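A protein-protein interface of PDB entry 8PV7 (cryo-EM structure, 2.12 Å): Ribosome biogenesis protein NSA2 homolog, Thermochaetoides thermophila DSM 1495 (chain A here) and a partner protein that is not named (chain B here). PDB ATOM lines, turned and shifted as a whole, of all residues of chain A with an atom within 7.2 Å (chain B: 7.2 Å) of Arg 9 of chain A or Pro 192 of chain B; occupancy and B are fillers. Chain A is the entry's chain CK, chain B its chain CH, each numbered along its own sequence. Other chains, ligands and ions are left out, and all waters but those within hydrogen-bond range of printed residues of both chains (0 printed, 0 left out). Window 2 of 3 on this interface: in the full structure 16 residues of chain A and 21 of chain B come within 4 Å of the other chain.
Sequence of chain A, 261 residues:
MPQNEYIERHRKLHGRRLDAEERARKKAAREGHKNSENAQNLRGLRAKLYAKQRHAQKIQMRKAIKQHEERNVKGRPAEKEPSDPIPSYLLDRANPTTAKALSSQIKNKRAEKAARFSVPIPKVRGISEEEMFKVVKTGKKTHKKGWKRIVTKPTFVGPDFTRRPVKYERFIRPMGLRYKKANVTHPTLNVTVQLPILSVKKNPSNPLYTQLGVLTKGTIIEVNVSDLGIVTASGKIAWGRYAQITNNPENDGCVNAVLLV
Of the 14 printed residues of chain B, 4 touch a printed residue of chain A. Hydrophobic or aromatic side chains of chain B within 4 Å of the printed part of chain A: Ala 189, Pro 192 and Phe 204.
O of Phe 204 of chain B is in hydrogen-bond range of N of Asp 219 of chain B (2.9 Å). OD1 of Asp 190 of chain B lies within salt-bridge range of NH1 of Arg 184 of chain B (2.8 Å).
The side-chain carboxylate (OD2) of Asp 190 of chain B lies within salt-bridge range of the guanidinium group (NE) of Arg 9 of chain A, at 3.1 Å.
Ala 189 of chain B touches Gln 3 of chain A (CB to NE2, 3.97 Å). Phe 204 of chain B touches Gln 3 of chain A. Arg 9 of chain A touches Pro 192 of chain B.
Printed residues of chain B within 4 Å of Gln 3 of chain A: Ala 189 (3.97 Å) and Phe 204 (3.4 Å). Tyr 6 of chain A touches none of the printed residues of chain B. Of chain B, only Asp 190 and Pro 192 come within 4 Å of Arg 9 of chain A. Of the printed residues of chain A, Ala 189 of chain B touches Gln 3. Of the printed residues of chain A, Asp 190 of chain B touches Arg 9. Printed residues of chain A within 4 Å of Pro 192 of chain B: Arg 9. Val 193 of chain B touches none of the printed residues of chain A. Printed residues of chain A within 4 Å of Phe 204 of chain B: Gln 3 (3.4 Å). The nearest printed residue of chain A that does not touch Ala 189 of chain B is Arg 9 of chain A (7.6 Å).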
ATOM      1  N   GLN A   3     -21.699 -14.618  30.070  1.00  0.00           N
ATOM      2  CA  GLN A   3     -20.854 -13.603  30.670  1.00  0.00           C
ATOM      3  C   GLN A   3     -21.110 -12.262  30.000  1.00  0.00           C
ATOM      4  O   GLN A   3     -21.449 -12.206  28.817  1.00  0.00           O
ATOM      5  CB  GLN A   3     -19.374 -13.971  30.541  1.00  0.00           C
ATOM      6  CG  GLN A   3     -19.004 -14.514  29.170  1.00  0.00           C
ATOM      7  CD  GLN A   3     -17.595 -15.062  29.101  1.00  0.00           C
ATOM      8  OE1 GLN A   3     -16.720 -14.643  29.850  1.00  0.00           O
ATOM      9  NE2 GLN A   3     -17.364 -15.985  28.190  1.00  0.00           N
ATOM     10  N   GLU A   5     -22.685  -8.837  28.738  1.00  0.00           N
ATOM     11  CA  GLU A   5     -24.034  -8.397  28.369  1.00  0.00           C
ATOM     12  C   GLU A   5     -24.685  -9.396  27.410  1.00  0.00           C
ATOM     13  O   GLU A   5     -24.942  -9.121  26.235  1.00  0.00           O
ATOM     14  CB  GLU A   5     -23.995  -6.994  27.781  1.00  0.00           C
ATOM     15  CG  GLU A   5     -23.957  -5.887  28.816  1.00  0.00           C
ATOM     16  CD  GLU A   5     -22.674  -5.865  29.619  1.00  0.00           C
ATOM     17  OE1 GLU A   5     -22.668  -6.360  30.769  1.00  0.00           O
ATOM     18  OE2 GLU A   5     -21.660  -5.367  29.094  1.00  0.00           O
ATOM     19  N   TYR A   6     -24.991 -10.574  27.958  1.00  0.00           N
ATOM     20  CA  TYR A   6     -25.337 -11.703  27.106  1.00  0.00           C
ATOM     21  C   TYR A   6     -26.756 -11.596  26.557  1.00  0.00           C
ATOM     22  O   TYR A   6     -27.017 -12.038  25.438  1.00  0.00           O
ATOM     23  CB  TYR A   6     -25.116 -13.026  27.845  1.00  0.00           C
ATOM     24  CG  TYR A   6     -25.707 -13.157  29.228  1.00  0.00           C
ATOM     25  CD1 TYR A   6     -26.986 -13.654  29.407  1.00  0.00           C
ATOM     26  CD2 TYR A   6     -24.961 -12.848  30.355  1.00  0.00           C
ATOM     27  CE1 TYR A   6     -27.521 -13.805  30.663  1.00  0.00           C
ATOM     28  CE2 TYR A   6     -25.486 -12.997  31.613  1.00  0.00           C
ATOM     29  CZ  TYR A   6     -26.763 -13.480  31.761  1.00  0.00           C
ATOM     30  OH  TYR A   6     -27.293 -13.625  33.015  1.00  0.00           O
ATOM     31  N   ILE A   7     -27.681 -10.985  27.302  1.00  0.00           N
ATOM     32  CA  ILE A   7     -29.028 -10.788  26.760  1.00  0.00           C
ATOM     33  C   ILE A   7     -29.023  -9.715  25.669  1.00  0.00           C
ATOM     34  O   ILE A   7     -29.735  -9.843  24.666  1.00  0.00           O
ATOM     35  CB  ILE A   7     -30.035 -10.485  27.891  1.00  0.00           C
ATOM     36  CG1 ILE A   7     -30.292 -11.743  28.726  1.00  0.00           C
ATOM     37  CG2 ILE A   7     -31.368  -9.981  27.362  1.00  0.00           C
ATOM     38  CD1 ILE A   7     -30.865 -12.896  27.944  1.00  0.00           C
ATOM     39  N   GLU A   8     -28.203  -8.672  25.816  1.00  0.00           N
ATOM     40  CA  GLU A   8     -28.033  -7.701  24.734  1.00  0.00           C
ATOM     41  C   GLU A   8     -27.415  -8.342  23.496  1.00  0.00           C
ATOM     42  O   GLU A   8     -27.829  -8.049  22.368  1.00  0.00           O
ATOM     43  CB  GLU A   8     -27.177  -6.522  25.196  1.00  0.00           C
ATOM     44  CG  GLU A   8     -27.863  -5.604  26.187  1.00  0.00           C
ATOM     45  CD  GLU A   8     -26.916  -4.595  26.810  1.00  0.00           C
ATOM     46  OE1 GLU A   8     -25.848  -4.331  26.220  1.00  0.00           O
ATOM     47  OE2 GLU A   8     -27.226  -4.083  27.904  1.00  0.00           O
ATOM     48  N   ARG A   9     -26.434  -9.228  23.682  1.00  0.00           N
ATOM     49  CA  ARG A   9     -25.851  -9.921  22.537  1.00  0.00           C
ATOM     50  C   ARG A   9     -26.852 -10.879  21.901  1.00  0.00           C
ATOM     51  O   ARG A   9     -26.884 -11.030  20.676  1.00  0.00           O
ATOM     52  CB  ARG A   9     -24.575 -10.653  22.947  1.00  0.00           C
ATOM     53  CG  ARG A   9     -23.944 -11.467  21.831  1.00  0.00           C
ATOM     54  CD  ARG A   9     -22.440 -11.375  21.841  1.00  0.00           C
ATOM     55  NE  ARG A   9     -21.833 -12.159  20.771  1.00  0.00           N
ATOM     56  CZ  ARG A   9     -21.656 -11.729  19.531  1.00  0.00           C
ATOM     57  NH1 ARG A   9     -22.053 -10.528  19.153  1.00  0.00           N
ATOM     58  NH2 ARG A   9     -21.060 -12.523  18.650  1.00  0.00           N
ATOM     59  N   HIS A  10     -27.679 -11.530  22.718  1.00  0.00           N
ATOM     60  CA  HIS A  10     -28.718 -12.399  22.188  1.00  0.00           C
ATOM     61  C   HIS A  10     -29.738 -11.612  21.377  1.00  0.00           C
ATOM     62  O   HIS A  10     -30.217 -12.087  20.346  1.00  0.00           O
ATOM     63  CB  HIS A  10     -29.410 -13.146  23.325  1.00  0.00           C
ATOM     64  CG  HIS A  10     -30.422 -14.137  22.852  1.00  0.00           C
ATOM     65  ND1 HIS A  10     -30.089 -15.425  22.504  1.00  0.00           N
ATOM     66  CD2 HIS A  10     -31.753 -14.022  22.644  1.00  0.00           C
ATOM     67  CE1 HIS A  10     -31.172 -16.066  22.111  1.00  0.00           C
ATOM     68  NE2 HIS A  10     -32.196 -15.236  22.183  1.00  0.00           N
ATOM     69  N   ARG A  11     -30.088 -10.413  21.841  1.00  0.00           N
ATOM     70  CA  ARG A  11     -30.970  -9.536  21.079  1.00  0.00           C
ATOM     71  C   ARG A  11     -30.328  -9.125  19.760  1.00  0.00           C
ATOM     72  O   ARG A  11     -31.002  -9.076  18.727  1.00  0.00           O
ATOM     73  CB  ARG A  11     -31.318  -8.308  21.917  1.00  0.00           C
ATOM     74  CG  ARG A  11     -32.210  -7.288  21.243  1.00  0.00           C
ATOM     75  CD  ARG A  11     -32.729  -6.290  22.261  1.00  0.00           C
ATOM     76  NE  ARG A  11     -33.542  -5.246  21.651  1.00  0.00           N
ATOM     77  CZ  ARG A  11     -34.712  -4.829  22.116  1.00  0.00           C
ATOM     78  NH1 ARG A  11     -35.242  -5.339  23.215  1.00  0.00           N
ATOM     79  NH2 ARG A  11     -35.371  -3.881  21.457  1.00  0.00           N
ATOM     80  N   LYS A  12     -29.024  -8.843  19.776  1.00  0.00           N
ATOM     81  CA  LYS A  12     -28.315  -8.491  18.548  1.00  0.00           C
ATOM     82  C   LYS A  12     -28.281  -9.649  17.554  1.00  0.00           C
ATOM     83  O   LYS A  12     -28.446  -9.443  16.348  1.00  0.00           O
ATOM     84  CB  LYS A  12     -26.899  -8.032  18.883  1.00  0.00           C
ATOM     85  CG  LYS A  12     -26.151  -7.409  17.722  1.00  0.00           C
ATOM     86  CD  LYS A  12     -24.729  -7.044  18.115  1.00  0.00           C
ATOM     87  CE  LYS A  12     -24.052  -6.195  17.054  1.00  0.00           C
ATOM     88  NZ  LYS A  12     -24.681  -4.853  16.925  1.00  0.00           N
ATOM     89  N   LEU A  13     -28.064 -10.872  18.035  1.00  0.00           N
ATOM     90  CA  LEU A  13     -27.910 -12.007  17.132  1.00  0.00           C
ATOM     91  C   LEU A  13     -29.239 -12.579  16.655  1.00  0.00           C
ATOM     92  O   LEU A  13     -29.338 -13.006  15.502  1.00  0.00           O
ATOM     93  CB  LEU A  13     -27.100 -13.113  17.803  1.00  0.00           C
ATOM     94  CG  LEU A  13     -25.620 -12.834  18.053  1.00  0.00           C
ATOM     95  CD1 LEU A  13     -24.989 -13.990  18.803  1.00  0.00           C
ATOM     96  CD2 LEU A  13     -24.899 -12.571  16.751  1.00  0.00           C
ATOM     97  N   HIS A  14     -30.261 -12.603  17.507  1.00  0.00           N
ATOM     98  CA  HIS A  14     -31.490 -13.319  17.206  1.00  0.00           C
ATOM     99  C   HIS A  14     -32.744 -12.461  17.251  1.00  0.00           C
ATOM    100  O   HIS A  14     -33.824 -12.974  16.952  1.00  0.00           O
ATOM    101  CB  HIS A  14     -31.666 -14.504  18.171  1.00  0.00           C
ATOM    102  CG  HIS A  14     -30.469 -15.395  18.256  1.00  0.00           C
ATOM    103  ND1 HIS A  14     -29.555 -15.321  19.284  1.00  0.00           N
ATOM    104  CD2 HIS A  14     -30.022 -16.367  17.427  1.00  0.00           C
ATOM    105  CE1 HIS A  14     -28.605 -16.215  19.091  1.00  0.00           C
ATOM    106  NE2 HIS A  14     -28.863 -16.862  17.969  1.00  0.00           N
ATOM    107  N   GLY A  15     -32.644 -11.190  17.612  1.00  0.00           N
ATOM    108  CA  GLY A  15     -33.826 -10.361  17.701  1.00  0.00           C
ATOM    109  C   GLY A  15     -34.662 -10.691  18.923  1.00  0.00           C
ATOM    110  O   GLY A  15     -34.182 -11.228  19.922  1.00  0.00           O
ATOM    111  N   SER B 180      -9.502 -11.687  20.222  1.00  0.00           N
ATOM    112  CA  SER B 180     -10.790 -12.363  20.284  1.00  0.00           C
ATOM    113  C   SER B 180     -10.928 -13.424  19.206  1.00  0.00           C
ATOM    114  O   SER B 180     -11.613 -14.425  19.422  1.00  0.00           O
ATOM    115  CB  SER B 180     -11.931 -11.361  20.158  1.00  0.00           C
ATOM    116  OG  SER B 180     -12.232 -10.775  21.405  1.00  0.00           O
ATOM    117  N   SER B 181     -10.297 -13.222  18.046  1.00  0.00           N
ATOM    118  CA  SER B 181     -10.314 -14.244  17.004  1.00  0.00           C
ATOM    119  C   SER B 181      -9.617 -15.516  17.460  1.00  0.00           C
ATOM    120  O   SER B 181     -10.136 -16.617  17.248  1.00  0.00           O
ATOM    121  CB  SER B 181      -9.652 -13.714  15.734  1.00  0.00           C
ATOM    122  OG  SER B 181     -10.412 -12.682  15.141  1.00  0.00           O
ATOM    123  N   ARG B 184     -11.859 -17.201  20.165  1.00  0.00           N
ATOM    124  CA  ARG B 184     -12.961 -17.899  19.508  1.00  0.00           C
ATOM    125  C   ARG B 184     -12.497 -19.159  18.795  1.00  0.00           C
ATOM    126  O   ARG B 184     -13.244 -20.139  18.734  1.00  0.00           O
ATOM    127  CB  ARG B 184     -13.655 -16.999  18.488  1.00  0.00           C
ATOM    128  CG  ARG B 184     -14.502 -15.903  19.053  1.00  0.00           C
ATOM    129  CD  ARG B 184     -15.344 -15.276  17.958  1.00  0.00           C
ATOM    130  NE  ARG B 184     -16.516 -16.076  17.642  1.00  0.00           N
ATOM    131  CZ  ARG B 184     -17.696 -15.931  18.227  1.00  0.00           C
ATOM    132  NH1 ARG B 184     -17.889 -15.033  19.178  1.00  0.00           N
ATOM    133  NH2 ARG B 184     -18.705 -16.709  17.853  1.00  0.00           N
ATOM    134  N   ALA B 189     -16.105 -19.774  23.927  1.00  0.00           N
ATOM    135  CA  ALA B 189     -16.598 -18.491  24.415  1.00  0.00           C
ATOM    136  C   ALA B 189     -17.108 -17.628  23.270  1.00  0.00           C
ATOM    137  O   ALA B 189     -16.563 -17.652  22.164  1.00  0.00           O
ATOM    138  CB  ALA B 189     -15.497 -17.754  25.172  1.00  0.00           C
ATOM    139  N   ASP B 190     -18.167 -16.870  23.539  1.00  0.00           N
ATOM    140  CA  ASP B 190     -18.798 -16.023  22.527  1.00  0.00           C
ATOM    141  C   ASP B 190     -18.316 -14.578  22.672  1.00  0.00           C
ATOM    142  O   ASP B 190     -19.071 -13.657  22.975  1.00  0.00           O
ATOM    143  CB  ASP B 190     -20.315 -16.121  22.637  1.00  0.00           C
ATOM    144  CG  ASP B 190     -21.034 -15.449  21.482  1.00  0.00           C
ATOM    145  OD1 ASP B 190     -20.403 -15.223  20.431  1.00  0.00           O
ATOM    146  OD2 ASP B 190     -22.229 -15.131  21.632  1.00  0.00           O
ATOM    147  N   THR B 191     -17.019 -14.385  22.451  1.00  0.00           N
ATOM    148  CA  THR B 191     -16.446 -13.047  22.515  1.00  0.00           C
ATOM    149  C   THR B 191     -16.428 -12.439  21.114  1.00  0.00           C
ATOM    150  O   THR B 191     -15.843 -13.034  20.200  1.00  0.00           O
ATOM    151  CB  THR B 191     -15.048 -13.075  23.141  1.00  0.00           C
ATOM    152  OG1 THR B 191     -14.372 -11.837  22.897  1.00  0.00           O
ATOM    153  CG2 THR B 191     -14.200 -14.241  22.628  1.00  0.00           C
ATOM    154  N   PRO B 192     -17.083 -11.299  20.892  1.00  0.00           N
ATOM    155  CA  PRO B 192     -17.277 -10.796  19.523  1.00  0.00           C
ATOM    156  C   PRO B 192     -15.992 -10.363  18.827  1.00  0.00           C
ATOM    157  O   PRO B 192     -15.068  -9.836  19.444  1.00  0.00           O
ATOM    158  CB  PRO B 192     -18.218  -9.603  19.723  1.00  0.00           C
ATOM    159  CG  PRO B 192     -18.898  -9.870  21.004  1.00  0.00           C
ATOM    160  CD  PRO B 192     -17.901 -10.566  21.866  1.00  0.00           C
ATOM    161  N   VAL B 193     -15.976 -10.551  17.510  1.00  0.00           N
ATOM    162  CA  VAL B 193     -14.863 -10.175  16.646  1.00  0.00           C
ATOM    163  C   VAL B 193     -15.362  -9.112  15.681  1.00  0.00           C
ATOM    164  O   VAL B 193     -16.315  -9.350  14.931  1.00  0.00           O
ATOM    165  CB  VAL B 193     -14.307 -11.385  15.883  1.00  0.00           C
ATOM    166  CG1 VAL B 193     -13.437 -10.940  14.713  1.00  0.00           C
ATOM    167  CG2 VAL B 193     -13.534 -12.275  16.817  1.00  0.00           C
ATOM    168  N   GLU B 194     -14.729  -7.946  15.700  1.00  0.00           N
ATOM    169  CA  GLU B 194     -15.111  -6.817  14.866  1.00  0.00           C
ATOM    170  C   GLU B 194     -13.856  -6.056  14.464  1.00  0.00           C
ATOM    171  O   GLU B 194     -12.827  -6.155  15.139  1.00  0.00           O
ATOM    172  CB  GLU B 194     -16.083  -5.884  15.603  1.00  0.00           C
ATOM    173  CG  GLU B 194     -17.466  -6.442  15.906  1.00  0.00           C
ATOM    174  CD  GLU B 194     -18.388  -6.462  14.704  1.00  0.00           C
ATOM    175  OE1 GLU B 194     -18.047  -5.853  13.669  1.00  0.00           O
ATOM    176  OE2 GLU B 194     -19.465  -7.086  14.798  1.00  0.00           O
ATOM    177  N   TYR B 196     -13.219  -2.801  14.530  1.00  0.00           N
ATOM    178  CA  TYR B 196     -12.963  -1.536  15.200  1.00  0.00           C
ATOM    179  C   TYR B 196     -12.322  -1.758  16.564  1.00  0.00           C
ATOM    180  O   TYR B 196     -12.456  -2.824  17.164  1.00  0.00           O
ATOM    181  CB  TYR B 196     -14.253  -0.720  15.338  1.00  0.00           C
ATOM    182  CG  TYR B 196     -15.319  -1.337  16.208  1.00  0.00           C
ATOM    183  CD1 TYR B 196     -16.253  -2.208  15.675  1.00  0.00           C
ATOM    184  CD2 TYR B 196     -15.414  -1.026  17.558  1.00  0.00           C
ATOM    185  CE1 TYR B 196     -17.232  -2.764  16.464  1.00  0.00           C
ATOM    186  CE2 TYR B 196     -16.386  -1.581  18.352  1.00  0.00           C
ATOM    187  CZ  TYR B 196     -17.290  -2.452  17.801  1.00  0.00           C
ATOM    188  OH  TYR B 196     -18.271  -3.004  18.584  1.00  0.00           O
ATOM    189  N   THR B 199     -13.547  -3.525  20.605  1.00  0.00           N
ATOM    190  CA  THR B 199     -14.719  -4.382  20.491  1.00  0.00           C
ATOM    191  C   THR B 199     -14.976  -5.101  21.807  1.00  0.00           C
ATOM    192  O   THR B 199     -16.115  -5.169  22.279  1.00  0.00           O
ATOM    193  CB  THR B 199     -14.517  -5.392  19.362  1.00  0.00           C
ATOM    194  OG1 THR B 199     -14.358  -4.697  18.123  1.00  0.00           O
ATOM    195  CG2 THR B 199     -15.698  -6.337  19.260  1.00  0.00           C
ATOM    196  N   THR B 200     -13.917  -5.606  22.422  1.00  0.00           N
ATOM    197  CA  THR B 200     -13.987  -6.259  23.715  1.00  0.00           C
ATOM    198  C   THR B 200     -13.715  -5.234  24.806  1.00  0.00           C
ATOM    199  O   THR B 200     -12.647  -4.621  24.836  1.00  0.00           O
ATOM    200  CB  THR B 200     -12.977  -7.402  23.761  1.00  0.00           C
ATOM    201  OG1 THR B 200     -13.314  -8.359  22.754  1.00  0.00           O
ATOM    202  CG2 THR B 200     -12.964  -8.085  25.087  1.00  0.00           C
ATOM    203  N   PHE B 204     -13.295 -11.723  29.024  1.00  0.00           N
ATOM    204  CA  PHE B 204     -14.049 -12.902  28.627  1.00  0.00           C
ATOM    205  C   PHE B 204     -13.192 -14.118  28.941  1.00  0.00           C
ATOM    206  O   PHE B 204     -11.963 -14.043  28.877  1.00  0.00           O
ATOM    207  CB  PHE B 204     -14.390 -12.886  27.132  1.00  0.00           C
ATOM    208  CG  PHE B 204     -15.569 -12.018  26.761  1.00  0.00           C
ATOM    209  CD1 PHE B 204     -15.427 -10.646  26.635  1.00  0.00           C
ATOM    210  CD2 PHE B 204     -16.803 -12.584  26.485  1.00  0.00           C
ATOM    211  CE1 PHE B 204     -16.503  -9.853  26.264  1.00  0.00           C
ATOM    212  CE2 PHE B 204     -17.880 -11.797  26.111  1.00  0.00           C
ATOM    213  CZ  PHE B 204     -17.729 -10.430  26.000  1.00  0.00           C
ATOM    214  N   ASP B 219      -9.624 -13.677  27.234  1.00  0.00           N
ATOM    215  CA  ASP B 219      -9.640 -12.588  26.271  1.00  0.00           C
ATOM    216  C   ASP B 219      -9.795 -11.262  27.002  1.00  0.00           C
ATOM    217  O   ASP B 219     -10.631 -11.118  27.899  1.00  0.00           O
ATOM    218  CB  ASP B 219     -10.790 -12.777  25.278  1.00  0.00           C
ATOM    219  CG  ASP B 219     -10.836 -11.701  24.202  1.00  0.00           C
ATOM    220  OD1 ASP B 219      -9.801 -11.073  23.912  1.00  0.00           O
ATOM    221  OD2 ASP B 219     -11.926 -11.482  23.644  1.00  0.00           O
